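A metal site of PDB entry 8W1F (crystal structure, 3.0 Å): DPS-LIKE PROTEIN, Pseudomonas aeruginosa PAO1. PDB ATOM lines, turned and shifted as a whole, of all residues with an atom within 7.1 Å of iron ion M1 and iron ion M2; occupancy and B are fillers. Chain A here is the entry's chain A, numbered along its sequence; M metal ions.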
ATOM      1  N   ALA A  43      -0.899 -10.955 -17.385  1.00  0.00           N
ATOM      2  CA  ALA A  43      -1.189 -11.052 -18.813  1.00  0.00           C
ATOM      3  C   ALA A  43      -2.217 -12.150 -19.062  1.00  0.00           C
ATOM      4  O   ALA A  43      -3.150 -11.968 -19.844  1.00  0.00           O
ATOM      5  CB  ALA A  43       0.095 -11.319 -19.587  1.00  0.00           C
ATOM      6  N   THR A  46      -5.587 -10.890 -18.310  1.00  0.00           N
ATOM      7  CA  THR A  46      -5.997  -9.991 -19.383  1.00  0.00           C
ATOM      8  C   THR A  46      -6.488 -10.756 -20.600  1.00  0.00           C
ATOM      9  O   THR A  46      -7.523 -10.413 -21.190  1.00  0.00           O
ATOM     10  CB  THR A  46      -4.825  -9.086 -19.758  1.00  0.00           C
ATOM     11  OG1 THR A  46      -4.403  -8.369 -18.591  1.00  0.00           O
ATOM     12  CG2 THR A  46      -5.241  -8.107 -20.836  1.00  0.00           C
ATOM     13  N   GLU A  47      -5.767 -11.813 -20.991  1.00  0.00           N
ATOM     14  CA  GLU A  47      -6.175 -12.572 -22.170  1.00  0.00           C
ATOM     15  C   GLU A  47      -7.513 -13.247 -21.967  1.00  0.00           C
ATOM     16  O   GLU A  47      -8.321 -13.311 -22.893  1.00  0.00           O
ATOM     17  CB  GLU A  47      -5.100 -13.599 -22.550  1.00  0.00           C
ATOM     18  CG  GLU A  47      -3.741 -12.949 -22.851  1.00  0.00           C
ATOM     19  CD  GLU A  47      -3.792 -12.013 -24.063  1.00  0.00           C
ATOM     20  OE1 GLU A  47      -4.629 -12.247 -24.961  1.00  0.00           O
ATOM     21  OE2 GLU A  47      -3.022 -11.038 -24.113  1.00  0.00           O
ATOM     22  N   CYS A  50     -10.317 -10.575 -22.223  1.00  0.00           N
ATOM     23  CA  CYS A  50     -10.533 -10.197 -23.616  1.00  0.00           C
ATOM     24  C   CYS A  50     -11.187 -11.332 -24.397  1.00  0.00           C
ATOM     25  O   CYS A  50     -11.995 -11.081 -25.294  1.00  0.00           O
ATOM     26  CB  CYS A  50      -9.202  -9.748 -24.243  1.00  0.00           C
ATOM     27  SG  CYS A  50      -8.577  -8.090 -23.688  1.00  0.00           S
ATOM     28  N   TYR A  54     -14.788 -10.698 -26.336  1.00  0.00           N
ATOM     29  CA  TYR A  54     -14.943 -10.893 -27.778  1.00  0.00           C
ATOM     30  C   TYR A  54     -16.012 -11.935 -28.072  1.00  0.00           C
ATOM     31  O   TYR A  54     -16.777 -11.793 -29.021  1.00  0.00           O
ATOM     32  CB  TYR A  54     -13.607 -11.288 -28.375  1.00  0.00           C
ATOM     33  CG  TYR A  54     -12.722 -10.161 -28.845  1.00  0.00           C
ATOM     34  CD1 TYR A  54     -13.104  -9.318 -29.880  1.00  0.00           C
ATOM     35  CD2 TYR A  54     -11.471  -9.981 -28.294  1.00  0.00           C
ATOM     36  CE1 TYR A  54     -12.271  -8.310 -30.340  1.00  0.00           C
ATOM     37  CE2 TYR A  54     -10.619  -8.985 -28.761  1.00  0.00           C
ATOM     38  CZ  TYR A  54     -11.025  -8.158 -29.779  1.00  0.00           C
ATOM     39  OH  TYR A  54     -10.169  -7.168 -30.238  1.00  0.00           O
ATOM     40  N   HIS A  76     -10.436 -12.863 -33.198  1.00  0.00           N
ATOM     41  CA  HIS A  76      -9.642 -12.285 -32.130  1.00  0.00           C
ATOM     42  C   HIS A  76      -9.824 -13.057 -30.827  1.00  0.00           C
ATOM     43  O   HIS A  76      -8.850 -13.369 -30.152  1.00  0.00           O
ATOM     44  CB  HIS A  76      -9.999 -10.807 -31.939  1.00  0.00           C
ATOM     45  CG  HIS A  76      -9.596  -9.951 -33.101  1.00  0.00           C
ATOM     46  ND1 HIS A  76      -9.638  -8.569 -33.052  1.00  0.00           N
ATOM     47  CD2 HIS A  76      -9.158 -10.272 -34.346  1.00  0.00           C
ATOM     48  CE1 HIS A  76      -9.244  -8.084 -34.223  1.00  0.00           C
ATOM     49  NE2 HIS A  76      -8.947  -9.098 -35.025  1.00  0.00           N
ATOM     50  N   GLN A  79      -7.649 -16.030 -30.829  1.00  0.00           N
ATOM     51  CA  GLN A  79      -6.245 -15.646 -30.696  1.00  0.00           C
ATOM     52  C   GLN A  79      -5.917 -15.243 -29.269  1.00  0.00           C
ATOM     53  O   GLN A  79      -4.840 -15.570 -28.761  1.00  0.00           O
ATOM     54  CB  GLN A  79      -5.916 -14.508 -31.675  1.00  0.00           C
ATOM     55  CG  GLN A  79      -5.697 -15.048 -33.080  1.00  0.00           C
ATOM     56  CD  GLN A  79      -5.854 -14.026 -34.180  1.00  0.00           C
ATOM     57  OE1 GLN A  79      -6.125 -12.855 -33.950  1.00  0.00           O
ATOM     58  NE2 GLN A  79      -5.732 -14.487 -35.416  1.00  0.00           N
ATOM     59  N   GLU A  80      -6.831 -14.565 -28.581  1.00  0.00           N
ATOM     60  CA  GLU A  80      -6.571 -14.209 -27.191  1.00  0.00           C
ATOM     61  C   GLU A  80      -6.358 -15.459 -26.348  1.00  0.00           C
ATOM     62  O   GLU A  80      -5.528 -15.467 -25.432  1.00  0.00           O
ATOM     63  CB  GLU A  80      -7.710 -13.387 -26.610  1.00  0.00           C
ATOM     64  CG  GLU A  80      -8.024 -12.097 -27.338  1.00  0.00           C
ATOM     65  CD  GLU A  80      -6.845 -11.197 -27.542  1.00  0.00           C
ATOM     66  OE1 GLU A  80      -5.812 -11.342 -26.846  1.00  0.00           O
ATOM     67  OE2 GLU A  80      -6.968 -10.303 -28.386  1.00  0.00           O
ATOM     68  N   MET A  81      -7.127 -16.515 -26.619  1.00  0.00           N
ATOM     69  CA  MET A  81      -6.954 -17.753 -25.867  1.00  0.00           C
ATOM     70  C   MET A  81      -5.620 -18.435 -26.182  1.00  0.00           C
ATOM     71  O   MET A  81      -5.041 -19.068 -25.298  1.00  0.00           O
ATOM     72  CB  MET A  81      -8.123 -18.674 -26.137  1.00  0.00           C
ATOM     73  CG  MET A  81      -8.258 -19.774 -25.119  1.00  0.00           C
ATOM     74  SD  MET A  81      -8.971 -19.234 -23.579  1.00  0.00           S
ATOM     75  CE  MET A  81      -7.934 -20.227 -22.512  1.00  0.00           C
ATOM     76  N   GLN A  82      -5.127 -18.329 -27.431  1.00  0.00           N
ATOM     77  CA  GLN A  82      -3.796 -18.860 -27.742  1.00  0.00           C
ATOM     78  C   GLN A  82      -2.738 -18.151 -26.921  1.00  0.00           C
ATOM     79  O   GLN A  82      -1.809 -18.780 -26.399  1.00  0.00           O
ATOM     80  CB  GLN A  82      -3.482 -18.712 -29.213  1.00  0.00           C
ATOM     81  CG  GLN A  82      -4.240 -19.632 -30.117  1.00  0.00           C
ATOM     82  CD  GLN A  82      -4.236 -19.179 -31.582  1.00  0.00           C
ATOM     83  OE1 GLN A  82      -3.655 -18.138 -31.926  1.00  0.00           O
ATOM     84  NE2 GLN A  82      -4.877 -19.961 -32.437  1.00  0.00           N
ATOM     85  N   HIS A  83      -2.849 -16.820 -26.816  1.00  0.00           N
ATOM     86  CA  HIS A  83      -1.939 -16.081 -25.955  1.00  0.00           C
ATOM     87  C   HIS A  83      -2.031 -16.551 -24.521  1.00  0.00           C
ATOM     88  O   HIS A  83      -1.022 -16.678 -23.825  1.00  0.00           O
ATOM     89  CB  HIS A  83      -2.257 -14.589 -26.037  1.00  0.00           C
ATOM     90  CG  HIS A  83      -2.213 -14.039 -27.424  1.00  0.00           C
ATOM     91  ND1 HIS A  83      -2.875 -12.880 -27.774  1.00  0.00           N
ATOM     92  CD2 HIS A  83      -1.603 -14.495 -28.540  1.00  0.00           C
ATOM     93  CE1 HIS A  83      -2.671 -12.652 -29.068  1.00  0.00           C
ATOM     94  NE2 HIS A  83      -1.901 -13.613 -29.553  1.00  0.00           N
ATOM     95  N   ALA A  84      -3.255 -16.800 -24.054  1.00  0.00           N
ATOM     96  CA  ALA A  84      -3.434 -17.313 -22.699  1.00  0.00           C
ATOM     97  C   ALA A  84      -2.678 -18.621 -22.528  1.00  0.00           C
ATOM     98  O   ALA A  84      -2.010 -18.842 -21.513  1.00  0.00           O
ATOM     99  CB  ALA A  84      -4.908 -17.496 -22.396  1.00  0.00           C
ATOM    100  N   LEU A  87       1.105 -18.053 -22.367  1.00  0.00           N
ATOM    101  CA  LEU A  87       1.477 -17.516 -21.072  1.00  0.00           C
ATOM    102  C   LEU A  87       1.377 -18.565 -19.967  1.00  0.00           C
ATOM    103  O   LEU A  87       2.270 -18.677 -19.125  1.00  0.00           O
ATOM    104  CB  LEU A  87       0.594 -16.315 -20.755  1.00  0.00           C
ATOM    105  CG  LEU A  87       0.651 -15.127 -21.719  1.00  0.00           C
ATOM    106  CD1 LEU A  87      -0.579 -14.270 -21.498  1.00  0.00           C
ATOM    107  CD2 LEU A  87       1.929 -14.340 -21.501  1.00  0.00           C
ATOM    108  N   ASN A 126     -13.186  -2.907 -27.572  1.00  0.00           N
ATOM    109  CA  ASN A 126     -12.113  -3.776 -28.026  1.00  0.00           C
ATOM    110  C   ASN A 126     -10.887  -2.970 -28.397  1.00  0.00           C
ATOM    111  O   ASN A 126      -9.768  -3.326 -28.030  1.00  0.00           O
ATOM    112  CB  ASN A 126     -12.594  -4.642 -29.188  1.00  0.00           C
ATOM    113  CG  ASN A 126     -13.628  -5.657 -28.754  1.00  0.00           C
ATOM    114  OD1 ASN A 126     -13.586  -6.135 -27.624  1.00  0.00           O
ATOM    115  ND2 ASN A 126     -14.541  -5.993 -29.643  1.00  0.00           N
ATOM    116  N   ALA A 129      -9.043  -1.956 -25.360  1.00  0.00           N
ATOM    117  CA  ALA A 129      -8.314  -3.053 -24.741  1.00  0.00           C
ATOM    118  C   ALA A 129      -7.016  -3.351 -25.464  1.00  0.00           C
ATOM    119  O   ALA A 129      -5.985  -3.576 -24.840  1.00  0.00           O
ATOM    120  CB  ALA A 129      -9.184  -4.315 -24.709  1.00  0.00           C
ATOM    121  N   GLU A 130      -7.058  -3.356 -26.789  1.00  0.00           N
ATOM    122  CA  GLU A 130      -5.860  -3.655 -27.564  1.00  0.00           C
ATOM    123  C   GLU A 130      -4.769  -2.632 -27.284  1.00  0.00           C
ATOM    124  O   GLU A 130      -3.592  -2.991 -27.104  1.00  0.00           O
ATOM    125  CB  GLU A 130      -6.204  -3.697 -29.057  1.00  0.00           C
ATOM    126  CG  GLU A 130      -7.288  -4.727 -29.430  1.00  0.00           C
ATOM    127  CD  GLU A 130      -6.866  -6.150 -29.151  1.00  0.00           C
ATOM    128  OE1 GLU A 130      -5.670  -6.339 -28.856  1.00  0.00           O
ATOM    129  OE2 GLU A 130      -7.728  -7.055 -29.216  1.00  0.00           O
ATOM    130  N   ALA A 133      -3.193  -3.260 -23.910  1.00  0.00           N
ATOM    131  CA  ALA A 133      -2.297  -4.407 -23.947  1.00  0.00           C
ATOM    132  C   ALA A 133      -0.988  -4.042 -24.624  1.00  0.00           C
ATOM    133  O   ALA A 133       0.089  -4.431 -24.161  1.00  0.00           O
ATOM    134  CB  ALA A 133      -2.946  -5.563 -24.691  1.00  0.00           C
ATOM    135  N   TYR A 137       2.570  -4.609 -22.829  1.00  0.00           N
ATOM    136  CA  TYR A 137       3.515  -5.598 -23.312  1.00  0.00           C
ATOM    137  C   TYR A 137       4.788  -4.936 -23.802  1.00  0.00           C
ATOM    138  O   TYR A 137       5.864  -5.534 -23.701  1.00  0.00           O
ATOM    139  CB  TYR A 137       2.847  -6.457 -24.374  1.00  0.00           C
ATOM    140  CG  TYR A 137       1.661  -7.245 -23.822  1.00  0.00           C
ATOM    141  CD1 TYR A 137       1.529  -7.481 -22.452  1.00  0.00           C
ATOM    142  CD2 TYR A 137       0.663  -7.737 -24.654  1.00  0.00           C
ATOM    143  CE1 TYR A 137       0.463  -8.184 -21.947  1.00  0.00           C
ATOM    144  CE2 TYR A 137      -0.398  -8.444 -24.141  1.00  0.00           C
ATOM    145  CZ  TYR A 137      -0.498  -8.659 -22.788  1.00  0.00           C
ATOM    146  OH  TYR A 137      -1.554  -9.353 -22.241  1.00  0.00           O
ATOM    147  N   ILE A 158       3.035 -11.949 -28.956  1.00  0.00           N
ATOM    148  CA  ILE A 158       1.713 -11.510 -28.554  1.00  0.00           C
ATOM    149  C   ILE A 158       1.495 -10.039 -28.887  1.00  0.00           C
ATOM    150  O   ILE A 158       0.456  -9.645 -29.423  1.00  0.00           O
ATOM    151  CB  ILE A 158       1.496 -11.763 -27.051  1.00  0.00           C
ATOM    152  CG1 ILE A 158       1.407 -13.270 -26.788  1.00  0.00           C
ATOM    153  CG2 ILE A 158       0.257 -11.002 -26.568  1.00  0.00           C
ATOM    154  CD1 ILE A 158       1.442 -13.604 -25.340  1.00  0.00           C
ATOM    155  N   LEU A 159       2.488  -9.189 -28.569  1.00  0.00           N
ATOM    156  CA  LEU A 159       2.392  -7.772 -28.875  1.00  0.00           C
ATOM    157  C   LEU A 159       2.026  -7.556 -30.329  1.00  0.00           C
ATOM    158  O   LEU A 159       1.126  -6.782 -30.663  1.00  0.00           O
ATOM    159  CB  LEU A 159       3.732  -7.084 -28.561  1.00  0.00           C
ATOM    160  CG  LEU A 159       3.902  -5.643 -29.072  1.00  0.00           C
ATOM    161  CD1 LEU A 159       2.895  -4.673 -28.471  1.00  0.00           C
ATOM    162  CD2 LEU A 159       5.298  -5.174 -28.802  1.00  0.00           C
ATOM    163  N   GLN A 161       0.505  -9.368 -32.388  1.00  0.00           N
ATOM    164  CA  GLN A 161      -0.895  -9.719 -32.637  1.00  0.00           C
ATOM    165  C   GLN A 161      -1.840  -8.652 -32.110  1.00  0.00           C
ATOM    166  O   GLN A 161      -2.849  -8.353 -32.747  1.00  0.00           O
ATOM    167  CB  GLN A 161      -1.231 -11.053 -31.978  1.00  0.00           C
ATOM    168  CG  GLN A 161      -2.570 -11.592 -32.402  1.00  0.00           C
ATOM    169  CD  GLN A 161      -2.426 -12.757 -33.349  1.00  0.00           C
ATOM    170  OE1 GLN A 161      -1.908 -13.841 -32.985  1.00  0.00           O
ATOM    171  NE2 GLN A 161      -2.862 -12.553 -34.593  1.00  0.00           N
ATOM    172  N   GLU A 162      -1.536  -8.098 -30.927  1.00  0.00           N
ATOM    173  CA  GLU A 162      -2.391  -7.037 -30.374  1.00  0.00           C
ATOM    174  C   GLU A 162      -2.340  -5.791 -31.249  1.00  0.00           C
ATOM    175  O   GLU A 162      -3.358  -5.106 -31.416  1.00  0.00           O
ATOM    176  CB  GLU A 162      -1.965  -6.672 -28.949  1.00  0.00           C
ATOM    177  CG  GLU A 162      -1.861  -7.828 -27.959  1.00  0.00           C
ATOM    178  CD  GLU A 162      -3.078  -8.708 -27.910  1.00  0.00           C
ATOM    179  OE1 GLU A 162      -3.856  -8.694 -28.864  1.00  0.00           O
ATOM    180  OE2 GLU A 162      -3.261  -9.425 -26.895  1.00  0.00           O
ATOM    181  N   GLU A 163      -1.171  -5.473 -31.825  1.00  0.00           N
ATOM    182  CA  GLU A 163      -1.097  -4.341 -32.743  1.00  0.00           C
ATOM    183  C   GLU A 163      -1.997  -4.579 -33.965  1.00  0.00           C
ATOM    184  O   GLU A 163      -2.684  -3.670 -34.431  1.00  0.00           O
ATOM    185  CB  GLU A 163       0.345  -4.074 -33.185  1.00  0.00           C
ATOM    186  CG  GLU A 163       1.356  -3.658 -32.086  1.00  0.00           C
ATOM    187  CD  GLU A 163       2.619  -2.956 -32.678  1.00  0.00           C
ATOM    188  OE1 GLU A 163       2.471  -2.307 -33.731  1.00  0.00           O
ATOM    189  OE2 GLU A 163       3.746  -3.059 -32.102  1.00  0.00           O
ATOM    190  N   GLU A 164      -2.013  -5.807 -34.469  1.00  0.00           N
ATOM    191  CA  GLU A 164      -2.919  -6.146 -35.570  1.00  0.00           C
ATOM    192  C   GLU A 164      -4.377  -6.026 -35.147  1.00  0.00           C
ATOM    193  O   GLU A 164      -5.215  -5.551 -35.918  1.00  0.00           O
ATOM    194  CB  GLU A 164      -2.589  -7.552 -36.077  1.00  0.00           C
ATOM    195  CG  GLU A 164      -3.570  -8.150 -37.093  1.00  0.00           C
ATOM    196  CD  GLU A 164      -3.112  -9.513 -37.601  1.00  0.00           C
ATOM    197  OE1 GLU A 164      -1.895  -9.793 -37.591  1.00  0.00           O
ATOM    198  OE2 GLU A 164      -3.992 -10.307 -37.984  1.00  0.00           O
ATOM    199  N   HIS A 165      -4.711  -6.469 -33.925  1.00  0.00           N
ATOM    200  CA  HIS A 165      -6.099  -6.360 -33.469  1.00  0.00           C
ATOM    201  C   HIS A 165      -6.517  -4.894 -33.389  1.00  0.00           C
ATOM    202  O   HIS A 165      -7.626  -4.542 -33.805  1.00  0.00           O
ATOM    203  CB  HIS A 165      -6.269  -7.011 -32.097  1.00  0.00           C
ATOM    204  CG  HIS A 165      -6.164  -8.503 -32.099  1.00  0.00           C
ATOM    205  ND1 HIS A 165      -6.031  -9.243 -30.954  1.00  0.00           N
ATOM    206  CD2 HIS A 165      -6.181  -9.396 -33.122  1.00  0.00           C
ATOM    207  CE1 HIS A 165      -5.959 -10.523 -31.259  1.00  0.00           C
ATOM    208  NE2 HIS A 165      -6.049 -10.653 -32.566  1.00  0.00           N
ATOM    209  N   ALA A 166      -5.638  -4.045 -32.867  1.00  0.00           N
ATOM    210  CA  ALA A 166      -5.936  -2.618 -32.804  1.00  0.00           C
ATOM    211  C   ALA A 166      -6.125  -2.045 -34.204  1.00  0.00           C
ATOM    212  O   ALA A 166      -7.035  -1.240 -34.426  1.00  0.00           O
ATOM    213  CB  ALA A 166      -4.830  -1.898 -32.042  1.00  0.00           C
HETATM  214 FE    FE M   1      -3.870 -11.300 -26.563  1.00  0.00          FE
HETATM  215 FE    FE M   2      -5.962  -8.628 -28.835  1.00  0.00          FE
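The side-chain hydroxyl (OH) of Tyr 137 is in hydrogen-bond range of the side-chain carboxylate (OE2) of Glu 47, 2.9 Å away.
A ring nitrogen (NE2) of His 165 lies within hydrogen-bond range of the side-chain amide oxygen (OE1) of Gln 79 (2.6 Å).
ND1 of His 83 lies close to O of Gln 79 (3.5 Å).
A ring nitrogen (NE2) of His 83 sits at hydrogen-bond distance from the side-chain amide oxygen (OE1) of Gln 161.
The side-chain carboxylate of Glu 130 sits close to the side-chain hydroxyl of Tyr 54 (2.6 Å).
Of the 26 residues printed, 4 come within 4 Å of iron ion M2.
Along chain A the residues within 4 Å of iron ion M2 span positions 80 to 165.
Iron ion M1 is bound by the side-chain carboxylate (OE1) of Glu 80 (2.0 Å).
OE2 of Glu 162 is bound to iron ion M1 (2.0 Å).
Iron ion M1 is bound by OE1 of Glu 47 (2.0 Å).
Iron ion M1 is bound by a ring nitrogen (ND1) of His 83 (2.2 Å).
Slightly farther from iron ion M1 lies the side-chain carboxylate (OE2) of Glu 47 (2.6 Å).
Iron ion M2 is bound by OE2 of Glu 80, at 2.0 Å.
Iron ion M2 is bound by OE1 of Glu 162, at 2.1 Å.
Iron ion M2 is bound by ND1 of His 165 (2.2 Å).
OE1 of Glu 130 is bound to iron ion M2 (2.3 Å).
Iron ion M2 is bound by OE2 of Glu 130, 2.4 Å away.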
